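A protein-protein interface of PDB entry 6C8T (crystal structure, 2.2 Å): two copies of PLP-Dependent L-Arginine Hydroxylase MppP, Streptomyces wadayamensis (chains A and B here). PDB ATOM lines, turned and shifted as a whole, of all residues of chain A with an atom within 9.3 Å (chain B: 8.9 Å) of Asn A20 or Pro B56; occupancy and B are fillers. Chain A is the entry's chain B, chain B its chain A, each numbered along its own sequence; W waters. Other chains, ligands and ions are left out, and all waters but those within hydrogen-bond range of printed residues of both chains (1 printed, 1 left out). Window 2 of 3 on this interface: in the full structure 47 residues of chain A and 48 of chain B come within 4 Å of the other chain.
Of the 17 printed residues of chain A, 1 touches a printed residue of chain B. Of the 18 printed residues of chain B, 3 touch a printed residue of chain A. Printed residues of chain B that touch a printed residue of chain A: Pro B56, Val B57 and Gln B58. Hydrophobic or aromatic side chains of chain B that line the printed part of chain A: Pro B56 and Val B57. Among the printed residues, 3 pairs touch across the chains.
The backbone NH of Val B57 sits at hydrogen-bond distance from the side-chain amide oxygen of Asn A20, at 3.4 Å. The backbone NH (N) of Gln B58 is in hydrogen-bond range of the side-chain amide oxygen (OD1) of Asn A20 (2.8 Å).
Among the printed residues, merely in contact across the chains: Asn A20 with Pro B56.
No position is printed for both chains. Of the 3 pairs that touch across the chains among the printed residues, none has its exchanged pair printed and touching as well.
Of chain B, only Pro B56, Val B57 and Gln B58 come within 4 Å of Asn A20. Pro B56 touches just one residue of chain A: Asn A20 (3.3 Å). No residue of chain B comes within 4 Å of Ser A21. Of the printed residues of chain A, Gln B58 touches Asn A20 (2.8 Å). Glu B53 touches none of the printed residues of chain A. The nearest residue of chain B that does not touch Asn A20 is Gln B59 (4.8 Å). The nearest residue of chain A that does not touch Pro B56 is Leu A19 (5.1 Å).
The side-chain amide nitrogen (NE2) of Gln B58 lies within hydrogen-bond range of the side-chain hydroxyl (OG) of Ser B62 (3.1 Å).
Water W1 lies within hydrogen-bond range of O of Leu A19 and N of Val B57.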
ATOM      1  N   TRP A  14      25.791  -0.295 -18.953  1.00  0.00           N
ATOM      2  CA  TRP A  14      26.811  -0.385 -17.911  1.00  0.00           C
ATOM      3  C   TRP A  14      27.256   0.999 -17.476  1.00  0.00           C
ATOM      4  O   TRP A  14      27.528   1.228 -16.291  1.00  0.00           O
ATOM      5  CB  TRP A  14      28.021  -1.166 -18.404  1.00  0.00           C
ATOM      6  CG  TRP A  14      27.835  -2.636 -18.528  1.00  0.00           C
ATOM      7  CD1 TRP A  14      27.625  -3.336 -19.682  1.00  0.00           C
ATOM      8  CD2 TRP A  14      27.868  -3.604 -17.470  1.00  0.00           C
ATOM      9  NE1 TRP A  14      27.518  -4.675 -19.409  1.00  0.00           N
ATOM     10  CE2 TRP A  14      27.660  -4.869 -18.059  1.00  0.00           C
ATOM     11  CE3 TRP A  14      28.052  -3.525 -16.087  1.00  0.00           C
ATOM     12  CZ2 TRP A  14      27.636  -6.053 -17.309  1.00  0.00           C
ATOM     13  CZ3 TRP A  14      28.019  -4.690 -15.345  1.00  0.00           C
ATOM     14  CH2 TRP A  14      27.803  -5.943 -15.958  1.00  0.00           C
ATOM     15  N   GLU A  15      27.300   1.954 -18.415  1.00  0.00           N
ATOM     16  CA  GLU A  15      27.799   3.279 -18.073  1.00  0.00           C
ATOM     17  C   GLU A  15      26.798   4.045 -17.219  1.00  0.00           C
ATOM     18  O   GLU A  15      27.213   4.841 -16.368  1.00  0.00           O
ATOM     19  CB  GLU A  15      28.164   4.056 -19.346  1.00  0.00           C
ATOM     20  CG  GLU A  15      29.320   3.440 -20.110  1.00  0.00           C
ATOM     21  CD  GLU A  15      29.726   4.188 -21.389  1.00  0.00           C
ATOM     22  OE1 GLU A  15      28.968   5.030 -21.906  1.00  0.00           O
ATOM     23  OE2 GLU A  15      30.833   3.917 -21.890  1.00  0.00           O
ATOM     24  N   TYR A  16      25.489   3.804 -17.408  1.00  0.00           N
ATOM     25  CA  TYR A  16      24.490   4.473 -16.581  1.00  0.00           C
ATOM     26  C   TYR A  16      24.804   4.276 -15.105  1.00  0.00           C
ATOM     27  O   TYR A  16      24.697   5.215 -14.310  1.00  0.00           O
ATOM     28  CB  TYR A  16      23.070   3.952 -16.897  1.00  0.00           C
ATOM     29  CG  TYR A  16      22.510   4.372 -18.248  1.00  0.00           C
ATOM     30  CD1 TYR A  16      22.793   5.628 -18.781  1.00  0.00           C
ATOM     31  CD2 TYR A  16      21.684   3.514 -18.985  1.00  0.00           C
ATOM     32  CE1 TYR A  16      22.276   6.029 -20.004  1.00  0.00           C
ATOM     33  CE2 TYR A  16      21.146   3.904 -20.212  1.00  0.00           C
ATOM     34  CZ  TYR A  16      21.465   5.171 -20.713  1.00  0.00           C
ATOM     35  OH  TYR A  16      21.009   5.607 -21.918  1.00  0.00           O
ATOM     36  N   LEU A  17      25.241   3.065 -14.738  1.00  0.00           N
ATOM     37  CA  LEU A  17      25.460   2.720 -13.339  1.00  0.00           C
ATOM     38  C   LEU A  17      26.532   3.589 -12.683  1.00  0.00           C
ATOM     39  O   LEU A  17      26.520   3.753 -11.458  1.00  0.00           O
ATOM     40  CB  LEU A  17      25.840   1.242 -13.237  1.00  0.00           C
ATOM     41  CG  LEU A  17      24.825   0.272 -13.842  1.00  0.00           C
ATOM     42  CD1 LEU A  17      25.353  -1.122 -13.755  1.00  0.00           C
ATOM     43  CD2 LEU A  17      23.497   0.370 -13.125  1.00  0.00           C
ATOM     44  N   ALA A  18      27.462   4.151 -13.467  1.00  0.00           N
ATOM     45  CA  ALA A  18      28.578   4.935 -12.928  1.00  0.00           C
ATOM     46  C   ALA A  18      28.281   6.416 -12.784  1.00  0.00           C
ATOM     47  O   ALA A  18      29.034   7.120 -12.089  1.00  0.00           O
ATOM     48  CB  ALA A  18      29.811   4.819 -13.837  1.00  0.00           C
ATOM     49  N   LEU A  19      27.218   6.898 -13.434  1.00  0.00           N
ATOM     50  CA  LEU A  19      27.105   8.319 -13.749  1.00  0.00           C
ATOM     51  C   LEU A  19      27.078   9.197 -12.518  1.00  0.00           C
ATOM     52  O   LEU A  19      27.430  10.383 -12.605  1.00  0.00           O
ATOM     53  CB  LEU A  19      25.842   8.591 -14.572  1.00  0.00           C
ATOM     54  CG  LEU A  19      25.958   8.469 -16.083  1.00  0.00           C
ATOM     55  CD1 LEU A  19      24.670   8.946 -16.752  1.00  0.00           C
ATOM     56  CD2 LEU A  19      27.134   9.251 -16.575  1.00  0.00           C
ATOM     57  N   ASN A  20      26.640   8.664 -11.381  1.00  0.00           N
ATOM     58  CA  ASN A  20      26.483   9.476 -10.185  1.00  0.00           C
ATOM     59  C   ASN A  20      27.466   9.094  -9.082  1.00  0.00           C
ATOM     60  O   ASN A  20      27.273   9.453  -7.918  1.00  0.00           O
ATOM     61  CB  ASN A  20      25.034   9.378  -9.725  1.00  0.00           C
ATOM     62  CG  ASN A  20      24.075   9.792 -10.825  1.00  0.00           C
ATOM     63  OD1 ASN A  20      24.005  10.965 -11.171  1.00  0.00           O
ATOM     64  ND2 ASN A  20      23.378   8.827 -11.416  1.00  0.00           N
ATOM     65  N   SER A  21      28.555   8.434  -9.440  1.00  0.00           N
ATOM     66  CA  SER A  21      29.538   7.982  -8.477  1.00  0.00           C
ATOM     67  C   SER A  21      30.830   8.755  -8.701  1.00  0.00           C
ATOM     68  O   SER A  21      31.156   9.132  -9.831  1.00  0.00           O
ATOM     69  CB  SER A  21      29.752   6.463  -8.595  1.00  0.00           C
ATOM     70  OG  SER A  21      31.116   6.134  -8.536  1.00  0.00           O
ATOM     71  N   GLU A  22      31.552   9.015  -7.609  1.00  0.00           N
ATOM     72  CA  GLU A  22      32.775   9.802  -7.694  1.00  0.00           C
ATOM     73  C   GLU A  22      33.911   9.015  -8.323  1.00  0.00           C
ATOM     74  O   GLU A  22      34.838   9.622  -8.860  1.00  0.00           O
ATOM     75  CB  GLU A  22      33.201  10.288  -6.304  1.00  0.00           C
ATOM     76  CG  GLU A  22      32.219  11.240  -5.620  1.00  0.00           C
ATOM     77  CD  GLU A  22      32.352  12.682  -6.093  1.00  0.00           C
ATOM     78  OE1 GLU A  22      32.988  12.919  -7.142  1.00  0.00           O
ATOM     79  OE2 GLU A  22      31.821  13.581  -5.406  1.00  0.00           O
ATOM     80  N   LEU A  23      33.862   7.684  -8.256  1.00  0.00           N
ATOM     81  CA  LEU A  23      34.867   6.832  -8.875  1.00  0.00           C
ATOM     82  C   LEU A  23      34.275   6.184 -10.131  1.00  0.00           C
ATOM     83  O   LEU A  23      34.317   4.960 -10.313  1.00  0.00           O
ATOM     84  CB  LEU A  23      35.372   5.804  -7.863  1.00  0.00           C
ATOM     85  CG  LEU A  23      35.866   6.424  -6.538  1.00  0.00           C
ATOM     86  CD1 LEU A  23      36.299   5.351  -5.556  1.00  0.00           C
ATOM     87  CD2 LEU A  23      37.003   7.371  -6.730  1.00  0.00           C
ATOM     88  N   ASN A  24      33.680   7.017 -10.980  1.00  0.00           N
ATOM     89  CA  ASN A  24      33.284   6.624 -12.327  1.00  0.00           C
ATOM     90  C   ASN A  24      34.539   6.582 -13.179  1.00  0.00           C
ATOM     91  O   ASN A  24      35.127   7.624 -13.466  1.00  0.00           O
ATOM     92  CB  ASN A  24      32.251   7.617 -12.871  1.00  0.00           C
ATOM     93  CG  ASN A  24      32.016   7.487 -14.366  1.00  0.00           C
ATOM     94  OD1 ASN A  24      32.604   6.646 -15.042  1.00  0.00           O
ATOM     95  ND2 ASN A  24      31.139   8.325 -14.883  1.00  0.00           N
ATOM     96  N   ILE A  25      34.955   5.382 -13.574  1.00  0.00           N
ATOM     97  CA  ILE A  25      36.002   5.224 -14.590  1.00  0.00           C
ATOM     98  C   ILE A  25      35.450   4.420 -15.754  1.00  0.00           C
ATOM     99  O   ILE A  25      36.165   3.615 -16.371  1.00  0.00           O
ATOM    100  CB  ILE A  25      37.263   4.558 -14.028  1.00  0.00           C
ATOM    101  CG1 ILE A  25      36.922   3.280 -13.256  1.00  0.00           C
ATOM    102  CG2 ILE A  25      38.016   5.540 -13.142  1.00  0.00           C
ATOM    103  CD1 ILE A  25      38.132   2.377 -13.057  1.00  0.00           C
ATOM    104  N   ALA A  26      34.183   4.660 -16.078  1.00  0.00           N
ATOM    105  CA  ALA A  26      33.479   3.821 -17.026  1.00  0.00           C
ATOM    106  C   ALA A  26      33.336   4.506 -18.377  1.00  0.00           C
ATOM    107  O   ALA A  26      34.053   4.142 -19.318  1.00  0.00           O
ATOM    108  CB  ALA A  26      32.116   3.441 -16.466  1.00  0.00           C
ATOM    109  N   ASP A  27      32.438   5.498 -18.498  1.00  0.00           N
ATOM    110  CA  ASP A  27      32.227   6.104 -19.806  1.00  0.00           C
ATOM    111  C   ASP A  27      33.478   6.864 -20.235  1.00  0.00           C
ATOM    112  O   ASP A  27      34.263   7.343 -19.408  1.00  0.00           O
ATOM    113  CB  ASP A  27      31.020   7.035 -19.813  1.00  0.00           C
ATOM    114  CG  ASP A  27      31.188   8.212 -18.906  1.00  0.00           C
ATOM    115  OD1 ASP A  27      31.929   9.153 -19.282  1.00  0.00           O
ATOM    116  OD2 ASP A  27      30.553   8.202 -17.818  1.00  0.00           O
ATOM    117  N   ARG A  31      35.898  14.036 -18.216  1.00  0.00           N
ATOM    118  CA  ARG A  31      35.424  14.576 -16.951  1.00  0.00           C
ATOM    119  C   ARG A  31      36.557  15.085 -16.067  1.00  0.00           C
ATOM    120  O   ARG A  31      36.338  15.300 -14.876  1.00  0.00           O
ATOM    121  CB  ARG A  31      34.607  13.517 -16.195  1.00  0.00           C
ATOM    122  CG  ARG A  31      33.393  13.028 -16.971  1.00  0.00           C
ATOM    123  CD  ARG A  31      32.673  11.874 -16.290  1.00  0.00           C
ATOM    124  NE  ARG A  31      31.704  11.263 -17.199  1.00  0.00           N
ATOM    125  CZ  ARG A  31      30.530  11.804 -17.518  1.00  0.00           C
ATOM    126  NH1 ARG A  31      30.164  12.969 -16.994  1.00  0.00           N
ATOM    127  NH2 ARG A  31      29.718  11.183 -18.358  1.00  0.00           N
ATOM    128  N   HIS A 330      32.480   0.925  -4.755  1.00  0.00           N
ATOM    129  CA  HIS A 330      31.991   2.140  -5.390  1.00  0.00           C
ATOM    130  C   HIS A 330      32.880   2.590  -6.535  1.00  0.00           C
ATOM    131  O   HIS A 330      32.901   3.772  -6.873  1.00  0.00           O
ATOM    132  CB  HIS A 330      31.822   3.257  -4.362  1.00  0.00           C
ATOM    133  CG  HIS A 330      30.859   2.912  -3.276  1.00  0.00           C
ATOM    134  ND1 HIS A 330      31.213   2.147  -2.187  1.00  0.00           N
ATOM    135  CD2 HIS A 330      29.544   3.193  -3.130  1.00  0.00           C
ATOM    136  CE1 HIS A 330      30.161   1.989  -1.405  1.00  0.00           C
ATOM    137  NE2 HIS A 330      29.136   2.616  -1.953  1.00  0.00           N
ATOM    138  N   PHE A 332      33.493   2.116 -10.588  1.00  0.00           N
ATOM    139  CA  PHE A 332      32.692   1.695 -11.735  1.00  0.00           C
ATOM    140  C   PHE A 332      33.524   1.774 -13.002  1.00  0.00           C
ATOM    141  O   PHE A 332      33.858   2.871 -13.473  1.00  0.00           O
ATOM    142  CB  PHE A 332      31.424   2.531 -11.857  1.00  0.00           C
ATOM    143  CG  PHE A 332      30.423   2.241 -10.785  1.00  0.00           C
ATOM    144  CD1 PHE A 332      29.466   1.261 -10.970  1.00  0.00           C
ATOM    145  CD2 PHE A 332      30.453   2.924  -9.577  1.00  0.00           C
ATOM    146  CE1 PHE A 332      28.541   0.973  -9.982  1.00  0.00           C
ATOM    147  CE2 PHE A 332      29.534   2.642  -8.586  1.00  0.00           C
ATOM    148  CZ  PHE A 332      28.570   1.666  -8.791  1.00  0.00           C
ATOM    149  N   ALA B  50      29.843  25.189 -12.748  1.00  0.00           N
ATOM    150  CA  ALA B  50      30.457  24.633 -11.544  1.00  0.00           C
ATOM    151  C   ALA B  50      29.515  23.661 -10.859  1.00  0.00           C
ATOM    152  O   ALA B  50      29.925  22.574 -10.434  1.00  0.00           O
ATOM    153  CB  ALA B  50      30.851  25.764 -10.594  1.00  0.00           C
ATOM    154  N   GLU B  51      28.230  24.014 -10.774  1.00  0.00           N
ATOM    155  CA  GLU B  51      27.265  23.076 -10.199  1.00  0.00           C
ATOM    156  C   GLU B  51      27.229  21.785 -11.013  1.00  0.00           C
ATOM    157  O   GLU B  51      27.187  20.679 -10.453  1.00  0.00           O
ATOM    158  CB  GLU B  51      25.867  23.708 -10.129  1.00  0.00           C
ATOM    159  CG  GLU B  51      24.816  22.794  -9.504  1.00  0.00           C
ATOM    160  CD  GLU B  51      23.377  23.275  -9.664  1.00  0.00           C
ATOM    161  OE1 GLU B  51      23.140  24.374 -10.187  1.00  0.00           O
ATOM    162  OE2 GLU B  51      22.478  22.511  -9.275  1.00  0.00           O
ATOM    163  N   SER B  52      27.293  21.906 -12.340  1.00  0.00           N
ATOM    164  CA  SER B  52      27.179  20.722 -13.195  1.00  0.00           C
ATOM    165  C   SER B  52      28.388  19.821 -13.061  1.00  0.00           C
ATOM    166  O   SER B  52      28.267  18.605 -13.241  1.00  0.00           O
ATOM    167  CB  SER B  52      26.975  21.135 -14.654  1.00  0.00           C
ATOM    168  OG  SER B  52      25.768  21.883 -14.790  1.00  0.00           O
ATOM    169  N   GLU B  53      29.551  20.381 -12.721  1.00  0.00           N
ATOM    170  CA  GLU B  53      30.726  19.556 -12.488  1.00  0.00           C
ATOM    171  C   GLU B  53      30.712  18.866 -11.131  1.00  0.00           C
ATOM    172  O   GLU B  53      31.386  17.844 -10.960  1.00  0.00           O
ATOM    173  CB  GLU B  53      32.015  20.402 -12.542  1.00  0.00           C
ATOM    174  CG  GLU B  53      32.314  21.073 -13.851  1.00  0.00           C
ATOM    175  CD  GLU B  53      33.541  21.997 -13.755  1.00  0.00           C
ATOM    176  OE1 GLU B  53      34.582  21.676 -14.345  1.00  0.00           O
ATOM    177  OE2 GLU B  53      33.474  23.043 -13.073  1.00  0.00           O
ATOM    178  N   GLN B  54      30.028  19.445 -10.146  1.00  0.00           N
ATOM    179  CA  GLN B  54      30.126  18.981  -8.766  1.00  0.00           C
ATOM    180  C   GLN B  54      29.020  18.021  -8.363  1.00  0.00           C
ATOM    181  O   GLN B  54      29.256  17.134  -7.550  1.00  0.00           O
ATOM    182  CB  GLN B  54      30.102  20.192  -7.817  1.00  0.00           C
ATOM    183  CG  GLN B  54      31.386  21.038  -7.874  1.00  0.00           C
ATOM    184  CD  GLN B  54      32.608  20.258  -7.416  1.00  0.00           C
ATOM    185  OE1 GLN B  54      32.510  19.376  -6.559  1.00  0.00           O
ATOM    186  NE2 GLN B  54      33.762  20.582  -7.978  1.00  0.00           N
ATOM    187  N   ARG B  55      27.877  18.161  -8.892  1.00  0.00           N
ATOM    188  CA  ARG B  55      26.733  17.397  -8.429  1.00  0.00           C
ATOM    189  C   ARG B  55      26.446  16.201  -9.338  1.00  0.00           C
ATOM    190  O   ARG B  55      26.614  16.276 -10.554  1.00  0.00           O
ATOM    191  CB  ARG B  55      25.496  18.293  -8.402  1.00  0.00           C
ATOM    192  CG  ARG B  55      25.534  19.350  -7.357  1.00  0.00           C
ATOM    193  CD  ARG B  55      24.270  19.269  -6.523  1.00  0.00           C
ATOM    194  NE  ARG B  55      23.253  19.975  -7.222  1.00  0.00           N
ATOM    195  CZ  ARG B  55      21.941  19.746  -7.159  1.00  0.00           C
ATOM    196  NH1 ARG B  55      21.404  18.797  -6.398  1.00  0.00           N
ATOM    197  NH2 ARG B  55      21.167  20.507  -7.909  1.00  0.00           N
ATOM    198  N   PRO B  56      25.944  15.101  -8.795  1.00  0.00           N
ATOM    199  CA  PRO B  56      25.482  14.003  -9.657  1.00  0.00           C
ATOM    200  C   PRO B  56      24.416  14.473 -10.645  1.00  0.00           C
ATOM    201  O   PRO B  56      23.431  15.118 -10.275  1.00  0.00           O
ATOM    202  CB  PRO B  56      24.941  12.972  -8.661  1.00  0.00           C
ATOM    203  CG  PRO B  56      24.878  13.659  -7.338  1.00  0.00           C
ATOM    204  CD  PRO B  56      25.786  14.811  -7.358  1.00  0.00           C
ATOM    205  N   VAL B  57      24.647  14.171 -11.923  1.00  0.00           N
ATOM    206  CA  VAL B  57      23.696  14.537 -12.969  1.00  0.00           C
ATOM    207  C   VAL B  57      22.276  14.110 -12.596  1.00  0.00           C
ATOM    208  O   VAL B  57      21.309  14.836 -12.848  1.00  0.00           O
ATOM    209  CB  VAL B  57      24.141  13.944 -14.317  1.00  0.00           C
ATOM    210  CG1 VAL B  57      24.111  12.419 -14.291  1.00  0.00           C
ATOM    211  CG2 VAL B  57      23.245  14.451 -15.437  1.00  0.00           C
ATOM    212  N   GLN B  58      22.127  12.962 -11.942  1.00  0.00           N
ATOM    213  CA  GLN B  58      20.776  12.483 -11.634  1.00  0.00           C
ATOM    214  C   GLN B  58      20.008  13.487 -10.779  1.00  0.00           C
ATOM    215  O   GLN B  58      18.793  13.660 -10.933  1.00  0.00           O
ATOM    216  CB  GLN B  58      20.837  11.133 -10.922  1.00  0.00           C
ATOM    217  CG  GLN B  58      19.480  10.565 -10.555  1.00  0.00           C
ATOM    218  CD  GLN B  58      18.642  10.273 -11.778  1.00  0.00           C
ATOM    219  OE1 GLN B  58      18.987   9.413 -12.590  1.00  0.00           O
ATOM    220  NE2 GLN B  58      17.542  11.004 -11.929  1.00  0.00           N
ATOM    221  N   GLN B  59      20.691  14.147  -9.857  1.00  0.00           N
ATOM    222  CA  GLN B  59      20.009  15.116  -9.017  1.00  0.00           C
ATOM    223  C   GLN B  59      19.585  16.316  -9.839  1.00  0.00           C
ATOM    224  O   GLN B  59      18.470  16.825  -9.681  1.00  0.00           O
ATOM    225  CB  GLN B  59      20.919  15.530  -7.870  1.00  0.00           C
ATOM    226  CG  GLN B  59      21.101  14.444  -6.826  1.00  0.00           C
ATOM    227  CD  GLN B  59      21.978  14.886  -5.657  1.00  0.00           C
ATOM    228  OE1 GLN B  59      22.103  16.074  -5.363  1.00  0.00           O
ATOM    229  NE2 GLN B  59      22.600  13.926  -5.003  1.00  0.00           N
ATOM    230  N   ILE B  60      20.449  16.761 -10.756  1.00  0.00           N
ATOM    231  CA  ILE B  60      20.108  17.936 -11.536  1.00  0.00           C
ATOM    232  C   ILE B  60      18.947  17.604 -12.439  1.00  0.00           C
ATOM    233  O   ILE B  60      18.015  18.401 -12.593  1.00  0.00           O
ATOM    234  CB  ILE B  60      21.318  18.464 -12.326  1.00  0.00           C
ATOM    235  CG1 ILE B  60      22.422  18.907 -11.356  1.00  0.00           C
ATOM    236  CG2 ILE B  60      20.878  19.643 -13.248  1.00  0.00           C
ATOM    237  CD1 ILE B  60      23.750  19.315 -12.005  1.00  0.00           C
ATOM    238  N   GLU B  61      18.979  16.411 -13.040  1.00  0.00           N
ATOM    239  CA  GLU B  61      17.930  16.018 -13.967  1.00  0.00           C
ATOM    240  C   GLU B  61      16.595  15.895 -13.252  1.00  0.00           C
ATOM    241  O   GLU B  61      15.572  16.362 -13.760  1.00  0.00           O
ATOM    242  CB  GLU B  61      18.292  14.690 -14.651  1.00  0.00           C
ATOM    243  CG  GLU B  61      17.278  14.220 -15.660  1.00  0.00           C
ATOM    244  CD  GLU B  61      17.700  12.931 -16.386  1.00  0.00           C
ATOM    245  OE1 GLU B  61      18.356  12.085 -15.760  1.00  0.00           O
ATOM    246  OE2 GLU B  61      17.365  12.766 -17.578  1.00  0.00           O
ATOM    247  N   SER B  62      16.573  15.208 -12.106  1.00  0.00           N
ATOM    248  CA  SER B  62      15.326  15.086 -11.370  1.00  0.00           C
ATOM    249  C   SER B  62      14.762  16.456 -11.074  1.00  0.00           C
ATOM    250  O   SER B  62      13.553  16.674 -11.193  1.00  0.00           O
ATOM    251  CB  SER B  62      15.527  14.325 -10.061  1.00  0.00           C
ATOM    252  OG  SER B  62      15.748  12.962 -10.316  1.00  0.00           O
ATOM    253  N   GLU B  63      15.640  17.406 -10.740  1.00  0.00           N
ATOM    254  CA  GLU B  63      15.202  18.756 -10.412  1.00  0.00           C
ATOM    255  C   GLU B  63      14.687  19.472 -11.648  1.00  0.00           C
ATOM    256  O   GLU B  63      13.650  20.132 -11.594  1.00  0.00           O
ATOM    257  CB  GLU B  63      16.340  19.552  -9.775  1.00  0.00           C
ATOM    258  CG  GLU B  63      16.683  19.157  -8.352  1.00  0.00           C
ATOM    259  CD  GLU B  63      17.989  19.810  -7.869  1.00  0.00           C
ATOM    260  OE1 GLU B  63      18.408  19.503  -6.747  1.00  0.00           O
ATOM    261  OE2 GLU B  63      18.655  20.572  -8.621  1.00  0.00           O
ATOM    262  N   PRO B  81      13.560   7.498 -11.351  1.00  0.00           N
ATOM    263  CA  PRO B  81      14.630   7.598 -12.350  1.00  0.00           C
ATOM    264  C   PRO B  81      14.456   6.583 -13.465  1.00  0.00           C
ATOM    265  O   PRO B  81      14.105   5.428 -13.235  1.00  0.00           O
ATOM    266  CB  PRO B  81      15.895   7.325 -11.533  1.00  0.00           C
ATOM    267  CG  PRO B  81      15.569   7.827 -10.186  1.00  0.00           C
ATOM    268  CD  PRO B  81      14.085   7.588  -9.979  1.00  0.00           C
ATOM    269  N   PRO B 256      24.477  18.060 -18.231  1.00  0.00           N
ATOM    270  CA  PRO B 256      23.922  18.604 -16.981  1.00  0.00           C
ATOM    271  C   PRO B 256      23.742  20.112 -17.002  1.00  0.00           C
ATOM    272  O   PRO B 256      22.856  20.641 -16.317  1.00  0.00           O
ATOM    273  CB  PRO B 256      24.945  18.181 -15.917  1.00  0.00           C
ATOM    274  CG  PRO B 256      26.184  17.783 -16.661  1.00  0.00           C
ATOM    275  CD  PRO B 256      25.682  17.244 -17.994  1.00  0.00           C
ATOM    276  N   LEU B 259      20.380  20.665 -18.500  1.00  0.00           N
ATOM    277  CA  LEU B 259      19.416  20.305 -17.465  1.00  0.00           C
ATOM    278  C   LEU B 259      19.321  21.401 -16.402  1.00  0.00           C
ATOM    279  O   LEU B 259      18.226  21.778 -15.971  1.00  0.00           O
ATOM    280  CB  LEU B 259      19.827  18.987 -16.839  1.00  0.00           C
ATOM    281  CG  LEU B 259      19.284  17.607 -17.225  1.00  0.00           C
ATOM    282  CD1 LEU B 259      18.225  17.586 -18.268  1.00  0.00           C
ATOM    283  CD2 LEU B 259      20.379  16.634 -17.553  1.00  0.00           C
ATOM    284  N   ARG B 263      16.084  23.765 -15.552  1.00  0.00           N
ATOM    285  CA  ARG B 263      15.543  23.901 -14.213  1.00  0.00           C
ATOM    286  C   ARG B 263      15.389  25.372 -13.869  1.00  0.00           C
ATOM    287  O   ARG B 263      14.331  25.801 -13.399  1.00  0.00           O
ATOM    288  CB  ARG B 263      16.431  23.177 -13.192  1.00  0.00           C
ATOM    289  CG  ARG B 263      16.127  23.541 -11.731  1.00  0.00           C
ATOM    290  CD  ARG B 263      17.298  24.322 -11.124  1.00  0.00           C
ATOM    291  NE  ARG B 263      18.261  23.354 -10.702  1.00  0.00           N
ATOM    292  CZ  ARG B 263      19.574  23.529 -10.583  1.00  0.00           C
ATOM    293  NH1 ARG B 263      20.212  24.687 -10.807  1.00  0.00           N
ATOM    294  NH2 ARG B 263      20.257  22.478 -10.215  1.00  0.00           N
HETATM  295  O   HOH W   1      27.299  12.979 -12.430  1.00  0.00           O
